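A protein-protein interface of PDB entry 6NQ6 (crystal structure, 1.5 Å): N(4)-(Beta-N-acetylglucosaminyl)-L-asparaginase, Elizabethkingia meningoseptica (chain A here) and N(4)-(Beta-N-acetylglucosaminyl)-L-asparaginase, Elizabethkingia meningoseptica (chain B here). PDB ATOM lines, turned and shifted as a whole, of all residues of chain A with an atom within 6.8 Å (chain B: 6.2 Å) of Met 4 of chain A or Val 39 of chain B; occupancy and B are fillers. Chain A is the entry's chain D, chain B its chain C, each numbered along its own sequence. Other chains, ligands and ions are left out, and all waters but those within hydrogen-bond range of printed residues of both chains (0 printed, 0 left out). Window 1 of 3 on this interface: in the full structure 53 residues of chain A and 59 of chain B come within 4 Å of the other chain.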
ATOM      1  N   ILE A   2      11.309 -31.823   3.509  1.00  0.00           N
ATOM      2  CA  ILE A   2      10.437 -30.692   3.186  1.00  0.00           C
ATOM      3  C   ILE A   2      10.638 -29.676   4.289  1.00  0.00           C
ATOM      4  O   ILE A   2      10.549 -30.009   5.472  1.00  0.00           O
ATOM      5  CB  ILE A   2       8.973 -31.069   3.009  1.00  0.00           C
ATOM      6  CG1 ILE A   2       8.128 -29.816   2.665  1.00  0.00           C
ATOM      7  CG2 ILE A   2       8.418 -31.809   4.202  1.00  0.00           C
ATOM      8  CD1 ILE A   2       6.753 -30.191   2.138  1.00  0.00           C
ATOM      9  N   GLY A   3      10.835 -28.417   3.881  1.00  0.00           N
ATOM     10  CA  GLY A   3      10.743 -27.239   4.775  1.00  0.00           C
ATOM     11  C   GLY A   3       9.561 -26.429   4.385  1.00  0.00           C
ATOM     12  O   GLY A   3       9.227 -26.257   3.189  1.00  0.00           O
ATOM     13  N   MET A   4       8.913 -25.841   5.405  1.00  0.00           N
ATOM     14  CA  MET A   4       7.677 -25.059   5.191  1.00  0.00           C
ATOM     15  C   MET A   4       7.634 -23.926   6.188  1.00  0.00           C
ATOM     16  O   MET A   4       7.823 -24.124   7.393  1.00  0.00           O
ATOM     17  CB  MET A   4       6.402 -25.927   5.338  1.00  0.00           C
ATOM     18  CG  MET A   4       5.083 -25.201   5.139  1.00  0.00           C
ATOM     19  SD  MET A   4       3.594 -26.245   5.205  1.00  0.00           S
ATOM     20  CE  MET A   4       3.627 -26.850   3.542  1.00  0.00           C
ATOM     21  N   ILE A   5       7.389 -22.751   5.654  1.00  0.00           N
ATOM     22  CA  ILE A   5       7.261 -21.529   6.454  1.00  0.00           C
ATOM     23  C   ILE A   5       5.961 -20.794   6.148  1.00  0.00           C
ATOM     24  O   ILE A   5       5.503 -20.854   4.973  1.00  0.00           O
ATOM     25  CB  ILE A   5       8.474 -20.641   6.307  1.00  0.00           C
ATOM     26  CG1 ILE A   5       8.723 -20.303   4.846  1.00  0.00           C
ATOM     27  CG2 ILE A   5       9.696 -21.256   6.978  1.00  0.00           C
ATOM     28  CD1 ILE A   5       9.856 -19.353   4.577  1.00  0.00           C
ATOM     29  N   ALA A   6       5.294 -20.185   7.141  1.00  0.00           N
ATOM     30  CA  ALA A   6       4.053 -19.509   6.875  1.00  0.00           C
ATOM     31  C   ALA A   6       3.988 -18.232   7.703  1.00  0.00           C
ATOM     32  O   ALA A   6       4.516 -18.098   8.842  1.00  0.00           O
ATOM     33  CB  ALA A   6       2.935 -20.451   7.247  1.00  0.00           C
ATOM     34  N   SER A  14       5.711 -18.989  11.478  1.00  0.00           N
ATOM     35  CA  SER A  14       6.161 -20.293  12.093  1.00  0.00           C
ATOM     36  C   SER A  14       6.725 -21.163  10.975  1.00  0.00           C
ATOM     37  O   SER A  14       6.512 -20.862   9.780  1.00  0.00           O
ATOM     38  CB  SER A  14       5.063 -21.022  12.787  1.00  0.00           C
ATOM     39  OG  SER A  14       4.529 -20.290  13.919  1.00  0.00           O
ATOM     40  N   GLY A  15       7.453 -22.221  11.323  1.00  0.00           N
ATOM     41  CA  GLY A  15       8.009 -23.065  10.296  1.00  0.00           C
ATOM     42  C   GLY A  15       8.277 -24.418  10.818  1.00  0.00           C
ATOM     43  O   GLY A  15       8.341 -24.676  12.016  1.00  0.00           O
ATOM     44  N   ALA A  16       8.521 -25.336   9.891  1.00  0.00           N
ATOM     45  CA  ALA A  16       8.748 -26.748  10.129  1.00  0.00           C
ATOM     46  C   ALA A  16       9.684 -27.312   9.079  1.00  0.00           C
ATOM     47  O   ALA A  16       9.660 -26.916   7.916  1.00  0.00           O
ATOM     48  CB  ALA A  16       7.454 -27.521  10.037  1.00  0.00           C
ATOM     49  N   CYS A  17      10.467 -28.310   9.497  1.00  0.00           N
ATOM     50  CA  CYS A  17      11.435 -28.968   8.615  1.00  0.00           C
ATOM     51  C   CYS A  17      11.519 -30.428   9.018  1.00  0.00           C
ATOM     52  O   CYS A  17      11.682 -30.729  10.184  1.00  0.00           O
ATOM     53  CB  CYS A  17      12.774 -28.225   8.620  1.00  0.00           C
ATOM     54  SG  CYS A  17      13.968 -28.781   7.377  1.00  0.00           S
ATOM     55  N   THR A  18      11.317 -31.359   8.070  1.00  0.00           N
ATOM     56  CA  THR A  18      11.295 -32.762   8.397  1.00  0.00           C
ATOM     57  C   THR A  18      11.914 -33.565   7.240  1.00  0.00           C
ATOM     58  O   THR A  18      11.671 -33.296   6.079  1.00  0.00           O
ATOM     59  CB  THR A  18       9.827 -33.199   8.719  1.00  0.00           C
ATOM     60  OG1 THR A  18       9.806 -34.600   9.113  1.00  0.00           O
ATOM     61  CG2 THR A  18       8.859 -32.899   7.623  1.00  0.00           C
ATOM     62  N   LEU A  40      16.185 -24.401   9.463  1.00  0.00           N
ATOM     63  CA  LEU A  40      15.005 -23.573   9.762  1.00  0.00           C
ATOM     64  C   LEU A  40      15.335 -22.453  10.717  1.00  0.00           C
ATOM     65  O   LEU A  40      15.961 -22.687  11.713  1.00  0.00           O
ATOM     66  CB  LEU A  40      13.896 -24.467  10.354  1.00  0.00           C
ATOM     67  CG  LEU A  40      12.621 -23.776  10.838  1.00  0.00           C
ATOM     68  CD1 LEU A  40      11.859 -23.302   9.616  1.00  0.00           C
ATOM     69  CD2 LEU A  40      11.733 -24.692  11.636  1.00  0.00           C
ATOM     70  N   VAL A  42      13.166 -18.809  12.436  1.00  0.00           N
ATOM     71  CA  VAL A  42      12.020 -17.931  12.442  1.00  0.00           C
ATOM     72  C   VAL A  42      12.225 -16.830  13.477  1.00  0.00           C
ATOM     73  O   VAL A  42      12.358 -17.138  14.678  1.00  0.00           O
ATOM     74  CB  VAL A  42      10.689 -18.669  12.773  1.00  0.00           C
ATOM     75  CG1 VAL A  42       9.490 -17.687  12.850  1.00  0.00           C
ATOM     76  CG2 VAL A  42      10.467 -19.787  11.817  1.00  0.00           C
ATOM     77  N   THR A  50      13.741 -21.367   5.366  1.00  0.00           N
ATOM     78  CA  THR A  50      13.996 -22.819   5.460  1.00  0.00           C
ATOM     79  C   THR A  50      14.852 -23.195   4.316  1.00  0.00           C
ATOM     80  O   THR A  50      14.905 -22.488   3.303  1.00  0.00           O
ATOM     81  CB  THR A  50      12.777 -23.755   5.483  1.00  0.00           C
ATOM     82  OG1 THR A  50      11.677 -23.182   6.144  1.00  0.00           O
ATOM     83  CG2 THR A  50      13.057 -25.018   6.040  1.00  0.00           C
ATOM     84  N   ILE A 107      14.296 -20.744   0.858  1.00  0.00           N
ATOM     85  CA  ILE A 107      13.078 -19.971   0.687  1.00  0.00           C
ATOM     86  C   ILE A 107      12.910 -19.109   1.932  1.00  0.00           C
ATOM     87  O   ILE A 107      13.314 -19.510   3.024  1.00  0.00           O
ATOM     88  CB  ILE A 107      11.825 -20.850   0.429  1.00  0.00           C
ATOM     89  CG1 ILE A 107      11.537 -21.788   1.566  1.00  0.00           C
ATOM     90  CG2 ILE A 107      12.065 -21.675  -0.772  1.00  0.00           C
ATOM     91  CD1 ILE A 107      10.288 -22.639   1.503  1.00  0.00           C
ATOM     92  N   VAL B   7       1.987 -19.232   2.620  1.00  0.00           N
ATOM     93  CA  VAL B   7       2.812 -20.354   2.994  1.00  0.00           C
ATOM     94  C   VAL B   7       3.711 -20.649   1.838  1.00  0.00           C
ATOM     95  O   VAL B   7       3.259 -20.672   0.659  1.00  0.00           O
ATOM     96  CB  VAL B   7       1.976 -21.562   3.420  1.00  0.00           C
ATOM     97  CG1 VAL B   7       0.967 -21.934   2.338  1.00  0.00           C
ATOM     98  CG2 VAL B   7       2.854 -22.776   3.794  1.00  0.00           C
ATOM     99  N   LEU B   8       4.970 -20.962   2.164  1.00  0.00           N
ATOM    100  CA  LEU B   8       6.036 -21.458   1.210  1.00  0.00           C
ATOM    101  C   LEU B   8       6.551 -22.770   1.624  1.00  0.00           C
ATOM    102  O   LEU B   8       6.729 -23.025   2.849  1.00  0.00           O
ATOM    103  CB  LEU B   8       7.219 -20.468   1.078  1.00  0.00           C
ATOM    104  CG  LEU B   8       7.066 -19.280   0.127  1.00  0.00           C
ATOM    105  CD1 LEU B   8       6.078 -18.270   0.670  1.00  0.00           C
ATOM    106  CD2 LEU B   8       8.454 -18.706   0.038  1.00  0.00           C
ATOM    107  N   SER B   9       6.837 -23.645   0.665  1.00  0.00           N
ATOM    108  CA  SER B   9       7.496 -24.898   0.975  1.00  0.00           C
ATOM    109  C   SER B   9       8.424 -25.338  -0.145  1.00  0.00           C
ATOM    110  O   SER B   9       8.312 -24.948  -1.298  1.00  0.00           O
ATOM    111  CB  SER B   9       6.508 -25.964   1.345  1.00  0.00           C
ATOM    112  OG  SER B   9       5.603 -26.233   0.286  1.00  0.00           O
ATOM    113  N   THR B  10       9.336 -26.185   0.223  1.00  0.00           N
ATOM    114  CA  THR B  10      10.395 -26.598  -0.669  1.00  0.00           C
ATOM    115  C   THR B  10       9.971 -27.744  -1.558  1.00  0.00           C
ATOM    116  O   THR B  10       9.313 -28.686  -1.103  1.00  0.00           O
ATOM    117  CB  THR B  10      11.600 -27.154   0.160  1.00  0.00           C
ATOM    118  OG1 THR B  10      11.178 -28.217   1.000  1.00  0.00           O
ATOM    119  CG2 THR B  10      12.252 -26.021   1.045  1.00  0.00           C
ATOM    120  N   GLY B  14       5.912 -29.669  -2.265  1.00  0.00           N
ATOM    121  CA  GLY B  14       5.327 -28.572  -1.531  1.00  0.00           C
ATOM    122  C   GLY B  14       4.031 -28.010  -2.078  1.00  0.00           C
ATOM    123  O   GLY B  14       3.235 -27.393  -1.340  1.00  0.00           O
ATOM    124  N   ALA B  17       1.417 -30.144  -0.350  1.00  0.00           N
ATOM    125  CA  ALA B  17       1.571 -29.845   1.079  1.00  0.00           C
ATOM    126  C   ALA B  17       0.937 -28.509   1.433  1.00  0.00           C
ATOM    127  O   ALA B  17       0.267 -28.380   2.439  1.00  0.00           O
ATOM    128  CB  ALA B  17       3.052 -29.852   1.431  1.00  0.00           C
ATOM    129  N   ASN B  18       1.143 -27.527   0.567  1.00  0.00           N
ATOM    130  CA  ASN B  18       0.590 -26.205   0.783  1.00  0.00           C
ATOM    131  C   ASN B  18      -0.943 -26.214   0.834  1.00  0.00           C
ATOM    132  O   ASN B  18      -1.551 -25.447   1.560  1.00  0.00           O
ATOM    133  CB  ASN B  18       0.958 -25.200  -0.320  1.00  0.00           C
ATOM    134  CG  ASN B  18       2.362 -24.598  -0.170  1.00  0.00           C
ATOM    135  OD1 ASN B  18       3.105 -24.931   0.781  1.00  0.00           O
ATOM    136  ND2 ASN B  18       2.697 -23.695  -1.097  1.00  0.00           N
ATOM    137  N   ALA B  21      -1.836 -27.044   4.341  1.00  0.00           N
ATOM    138  CA  ALA B  21      -1.545 -25.917   5.199  1.00  0.00           C
ATOM    139  C   ALA B  21      -2.570 -24.805   5.068  1.00  0.00           C
ATOM    140  O   ALA B  21      -2.980 -24.183   6.056  1.00  0.00           O
ATOM    141  CB  ALA B  21      -0.135 -25.398   4.885  1.00  0.00           C
ATOM    142  N   ALA B  34      -0.635 -24.711  10.794  1.00  0.00           N
ATOM    143  CA  ALA B  34      -0.590 -24.834   9.306  1.00  0.00           C
ATOM    144  C   ALA B  34       0.659 -25.589   8.870  1.00  0.00           C
ATOM    145  O   ALA B  34       0.538 -26.482   8.032  1.00  0.00           O
ATOM    146  CB  ALA B  34      -0.707 -23.484   8.655  1.00  0.00           C
ATOM    147  N   VAL B  35       1.835 -25.192   9.385  1.00  0.00           N
ATOM    148  CA  VAL B  35       3.072 -25.804   8.894  1.00  0.00           C
ATOM    149  C   VAL B  35       3.196 -27.241   9.423  1.00  0.00           C
ATOM    150  O   VAL B  35       3.737 -28.082   8.732  1.00  0.00           O
ATOM    151  CB  VAL B  35       4.307 -24.923   9.187  1.00  0.00           C
ATOM    152  CG1 VAL B  35       4.173 -23.577   8.589  1.00  0.00           C
ATOM    153  CG2 VAL B  35       4.606 -24.857  10.697  1.00  0.00           C
ATOM    154  N   GLU B  36       2.720 -27.541  10.620  1.00  0.00           N
ATOM    155  CA  GLU B  36       2.735 -28.917  11.106  1.00  0.00           C
ATOM    156  C   GLU B  36       1.808 -29.814  10.258  1.00  0.00           C
ATOM    157  O   GLU B  36       2.254 -30.874   9.752  1.00  0.00           O
ATOM    158  CB  GLU B  36       2.276 -28.972  12.572  1.00  0.00           C
ATOM    159  CG  GLU B  36       2.304 -30.389  13.123  1.00  0.00           C
ATOM    160  CD  GLU B  36       1.676 -30.573  14.483  1.00  0.00           C
ATOM    161  OE1 GLU B  36       0.918 -29.690  14.903  1.00  0.00           O
ATOM    162  OE2 GLU B  36       1.976 -31.615  15.108  1.00  0.00           O
ATOM    163  N   LYS B  37       0.602 -29.336   9.960  1.00  0.00           N
ATOM    164  CA  LYS B  37      -0.315 -30.179   9.103  1.00  0.00           C
ATOM    165  C   LYS B  37       0.262 -30.357   7.688  1.00  0.00           C
ATOM    166  O   LYS B  37       0.140 -31.481   7.102  1.00  0.00           O
ATOM    167  CB  LYS B  37      -1.740 -29.623   9.063  1.00  0.00           C
ATOM    168  CG  LYS B  37      -2.477 -29.749  10.383  1.00  0.00           C
ATOM    169  CD  LYS B  37      -3.994 -29.660  10.207  1.00  0.00           C
ATOM    170  CE  LYS B  37      -4.743 -30.651  11.084  1.00  0.00           C
ATOM    171  NZ  LYS B  37      -4.488 -30.404  12.494  1.00  0.00           N
ATOM    172  N   GLY B  38       0.805 -29.273   7.134  1.00  0.00           N
ATOM    173  CA  GLY B  38       1.308 -29.355   5.789  1.00  0.00           C
ATOM    174  C   GLY B  38       2.421 -30.349   5.687  1.00  0.00           C
ATOM    175  O   GLY B  38       2.458 -31.107   4.684  1.00  0.00           O
ATOM    176  N   VAL B  39       3.415 -30.339   6.603  1.00  0.00           N
ATOM    177  CA  VAL B  39       4.532 -31.285   6.377  1.00  0.00           C
ATOM    178  C   VAL B  39       4.140 -32.696   6.771  1.00  0.00           C
ATOM    179  O   VAL B  39       4.691 -33.648   6.225  1.00  0.00           O
ATOM    180  CB  VAL B  39       5.860 -30.810   7.026  1.00  0.00           C
ATOM    181  CG1 VAL B  39       6.275 -29.450   6.489  1.00  0.00           C
ATOM    182  CG2 VAL B  39       5.852 -30.921   8.533  1.00  0.00           C
ATOM    183  N   ARG B  40       3.171 -32.828   7.652  1.00  0.00           N
ATOM    184  CA  ARG B  40       2.674 -34.186   8.042  1.00  0.00           C
ATOM    185  C   ARG B  40       2.114 -34.943   6.824  1.00  0.00           C
ATOM    186  O   ARG B  40       2.285 -36.141   6.701  1.00  0.00           O
ATOM    187  CB  ARG B  40       1.623 -34.084   9.112  1.00  0.00           C
ATOM    188  CG  ARG B  40       2.118 -33.975  10.582  1.00  0.00           C
ATOM    189  CD  ARG B  40       0.947 -33.829  11.556  1.00  0.00           C
ATOM    190  NE  ARG B  40       0.143 -35.048  11.511  1.00  0.00           N
ATOM    191  CZ  ARG B  40       0.240 -36.024  12.406  1.00  0.00           C
ATOM    192  NH1 ARG B  40       1.052 -36.002  13.463  1.00  0.00           N
ATOM    193  NH2 ARG B  40      -0.551 -37.075  12.249  1.00  0.00           N
ATOM    194  N   LEU B  41       1.511 -34.219   5.897  1.00  0.00           N
ATOM    195  CA  LEU B  41       0.954 -34.841   4.693  1.00  0.00           C
ATOM    196  C   LEU B  41       2.062 -35.595   3.950  1.00  0.00           C
ATOM    197  O   LEU B  41       1.861 -36.694   3.372  1.00  0.00           O
ATOM    198  CB  LEU B  41       0.387 -33.752   3.768  1.00  0.00           C
ATOM    199  CG  LEU B  41      -0.305 -34.323   2.508  1.00  0.00           C
ATOM    200  CD1 LEU B  41      -1.701 -34.967   2.774  1.00  0.00           C
ATOM    201  CD2 LEU B  41      -0.348 -33.217   1.447  1.00  0.00           C
ATOM    202  N   VAL B  42       3.258 -35.003   3.882  1.00  0.00           N
ATOM    203  CA  VAL B  42       4.373 -35.599   3.177  1.00  0.00           C
ATOM    204  C   VAL B  42       5.065 -36.678   3.995  1.00  0.00           C
ATOM    205  O   VAL B  42       5.484 -37.699   3.434  1.00  0.00           O
ATOM    206  CB  VAL B  42       5.357 -34.492   2.750  1.00  0.00           C
ATOM    207  CG1 VAL B  42       6.490 -35.094   1.924  1.00  0.00           C
ATOM    208  CG2 VAL B  42       4.673 -33.413   1.920  1.00  0.00           C
ATOM    209  N   GLU B  43       5.179 -36.483   5.319  1.00  0.00           N
ATOM    210  CA  GLU B  43       5.605 -37.543   6.232  1.00  0.00           C
ATOM    211  C   GLU B  43       4.799 -38.819   6.068  1.00  0.00           C
ATOM    212  O   GLU B  43       5.345 -39.933   6.087  1.00  0.00           O
ATOM    213  CB  GLU B  43       5.543 -37.089   7.685  1.00  0.00           C
ATOM    214  CG  GLU B  43       6.572 -36.035   8.080  1.00  0.00           C
ATOM    215  CD  GLU B  43       6.366 -35.555   9.522  1.00  0.00           C
ATOM    216  OE1 GLU B  43       5.311 -35.679  10.142  1.00  0.00           O
ATOM    217  OE2 GLU B  43       7.375 -35.056  10.158  1.00  0.00           O
ATOM    218  N   ASP B  44       3.493 -38.623   5.891  1.00  0.00           N
ATOM    219  CA  ASP B  44       2.544 -39.774   5.820  1.00  0.00           C
ATOM    220  C   ASP B  44       2.647 -40.519   4.520  1.00  0.00           C
ATOM    221  O   ASP B  44       2.238 -41.694   4.472  1.00  0.00           O
ATOM    222  CB  ASP B  44       1.113 -39.257   5.958  1.00  0.00           C
ATOM    223  CG  ASP B  44       0.770 -38.831   7.316  1.00  0.00           C
ATOM    224  OD1 ASP B  44       1.429 -39.189   8.280  1.00  0.00           O
ATOM    225  OD2 ASP B  44      -0.321 -38.184   7.443  1.00  0.00           O
ATOM    226  N   VAL B  51      11.137 -38.193   3.082  1.00  0.00           N
ATOM    227  CA  VAL B  51      10.469 -37.625   4.267  1.00  0.00           C
ATOM    228  C   VAL B  51       9.637 -38.707   4.903  1.00  0.00           C
ATOM    229  O   VAL B  51       8.848 -39.396   4.197  1.00  0.00           O
ATOM    230  CB  VAL B  51       9.530 -36.434   3.989  1.00  0.00           C
ATOM    231  CG1 VAL B  51       8.891 -35.903   5.268  1.00  0.00           C
ATOM    232  CG2 VAL B  51      10.200 -35.345   3.152  1.00  0.00           C
ATOM    233  N   ASN B  87       5.570 -39.341  12.287  1.00  0.00           N
ATOM    234  CA  ASN B  87       5.437 -37.854  12.261  1.00  0.00           C
ATOM    235  C   ASN B  87       6.391 -37.163  13.209  1.00  0.00           C
ATOM    236  O   ASN B  87       6.034 -36.625  14.254  1.00  0.00           O
ATOM    237  CB  ASN B  87       4.028 -37.532  12.580  1.00  0.00           C
ATOM    238  CG  ASN B  87       3.090 -38.100  11.565  1.00  0.00           C
ATOM    239  OD1 ASN B  87       3.049 -37.633  10.418  1.00  0.00           O
ATOM    240  ND2 ASN B  87       2.376 -39.152  11.958  1.00  0.00           N
ATOM    241  N   ILE B  89       7.791 -34.317  12.957  1.00  0.00           N
ATOM    242  CA  ILE B  89       7.446 -32.913  13.227  1.00  0.00           C
ATOM    243  C   ILE B  89       6.606 -32.776  14.447  1.00  0.00           C
ATOM    244  O   ILE B  89       6.765 -31.786  15.187  1.00  0.00           O
ATOM    245  CB  ILE B  89       6.843 -32.205  12.003  1.00  0.00           C
ATOM    246  CG1 ILE B  89       6.871 -30.671  12.183  1.00  0.00           C
ATOM    247  CG2 ILE B  89       5.466 -32.804  11.657  1.00  0.00           C
ATOM    248  CD1 ILE B  89       8.257 -30.093  12.301  1.00  0.00           C
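OD1 of Asn 18 of chain B sits at hydrogen-bond distance from OG of Ser 9 of chain B. O of Ala 16 of chain A is in hydrogen-bond range of N of Met 4 of chain A, at 2.8 Å. The side-chain carboxylate (OE2) of Glu 43 of chain B lies within hydrogen-bond range of the backbone NH (N) of Ile 89 of chain B, 2.9 Å away. The backbone carbonyl oxygen (O) of Gly 14 of chain B sits close to the side-chain amide oxygen (OD1) of Asn 18 of chain B, 3.3 Å away. The backbone NH (N) of Ile 2 of chain A lies within hydrogen-bond range of the backbone carbonyl oxygen (O) of Thr 18 of chain A (3.0 Å). The backbone NH of Thr 50 of chain A sits at hydrogen-bond distance from the backbone carbonyl oxygen of Ile 107 of chain A, at 3.0 Å.
The side-chain hydroxyl (OG1) of Thr 10 of chain B lies within hydrogen-bond range of the backbone NH (N) of Gly 3 of chain A, at 2.9 Å. The side-chain hydroxyl (OG1) of Thr 18 of chain A is in hydrogen-bond range of the side-chain carboxylate (OE2) of Glu 43 of chain B (2.7 Å). The backbone NH (N) of Leu 8 of chain B lies within hydrogen-bond range of the backbone carbonyl oxygen (O) of Ile 5 of chain A, at 2.9 Å.
Among the printed residues, merely in contact across the chains: Gly 3 of chain A with Ser 9 of chain B, Met 4 of chain A with Leu 8 of chain B, Ile 5 of chain A with Val 7 of chain B, Ile 2 of chain A with Thr 10 of chain B, Met 4 of chain A with Asn 18 of chain B, Ala 16 of chain A with Ile 89 of chain B, Met 4 of chain A with Val 7 of chain B, Ala 6 of chain A with Val 35 of chain B, Ile 107 of chain A with Ser 9 of chain B, Gly 15 of chain A with Val 35 of chain B, Thr 18 of chain A with Val 39 of chain B, Met 4 of chain A with Val 39 of chain B, Ile 2 of chain A with Val 51 of chain B, Met 4 of chain A with Ala 17 of chain B, Met 4 of chain A with Ser 9 of chain B, Ile 107 of chain A with Leu 8 of chain B, Met 4 of chain A with Val 35 of chain B, Ser 14 of chain A with Val 35 of chain B, Ile 2 of chain A with Ala 17 of chain B, Thr 18 of chain A with Val 51 of chain B, Met 4 of chain A with Ala 21 of chain B, Ile 2 of chain A with Val 42 of chain B, Ile 107 of chain A with Thr 10 of chain B, Met 4 of chain A with Gly 38 of chain B, Ile 2 of chain A with Val 39 of chain B, Ala 16 of chain A with Val 35 of chain B and Cys 17 of chain A with Ile 89 of chain B.
Of the printed residues of chain B, Gly 3 of chain A touches Ser 9 and Thr 10. Met 4 of chain A touches just these residues of chain B: Val 7 (3.6 Å), Leu 8 (3.2 Å), Ser 9 (3.7 Å), Ala 17 (3.7 Å), Asn 18 (3.4 Å), Ala 21 (3.8 Å), Val 35 (3.8 Å), Gly 38 (3.9 Å) and Val 39 (3.7 Å). Thr 50 of chain A touches none of the printed residues of chain B. Of the printed residues of chain A, Thr 10 of chain B touches Ile 2 (3.4 Å), Gly 3 (2.9 Å) and Ile 107 (3.9 Å). Of chain A, only Ile 2, Met 4 and Thr 18 come within 4 Å of Val 39 of chain B. Of the printed residues of chain A, Val 42 of chain B touches Ile 2. The nearest residue of chain B that does not touch Met 4 of chain A is Ala 34 of chain B (4.2 Å). The nearest printed residue of chain B that does not touch Gly 15 of chain A is Ile 89 of chain B (5.4 Å).
Of the 22 printed residues of chain B, 14 touch a printed residue of chain A. Printed residues of chain B that touch a printed residue of chain A: Val 7, Leu 8, Ser 9, Thr 10, Ala 17, Asn 18, Ala 21, Val 35, Gly 38, Val 39, Val 42, Glu 43, Val 51 and Ile 89. Printed residues of chain A that touch a printed residue of chain B: Ile 2, Gly 3, Met 4, Ile 5, Ala 6, Ser 14, Gly 15, Ala 16, Cys 17, Thr 18 and Ile 107. Among the printed residues, no Asp or Glu carboxylate lies within 4 Å of a Lys or Arg side-chain nitrogen of the other chain.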
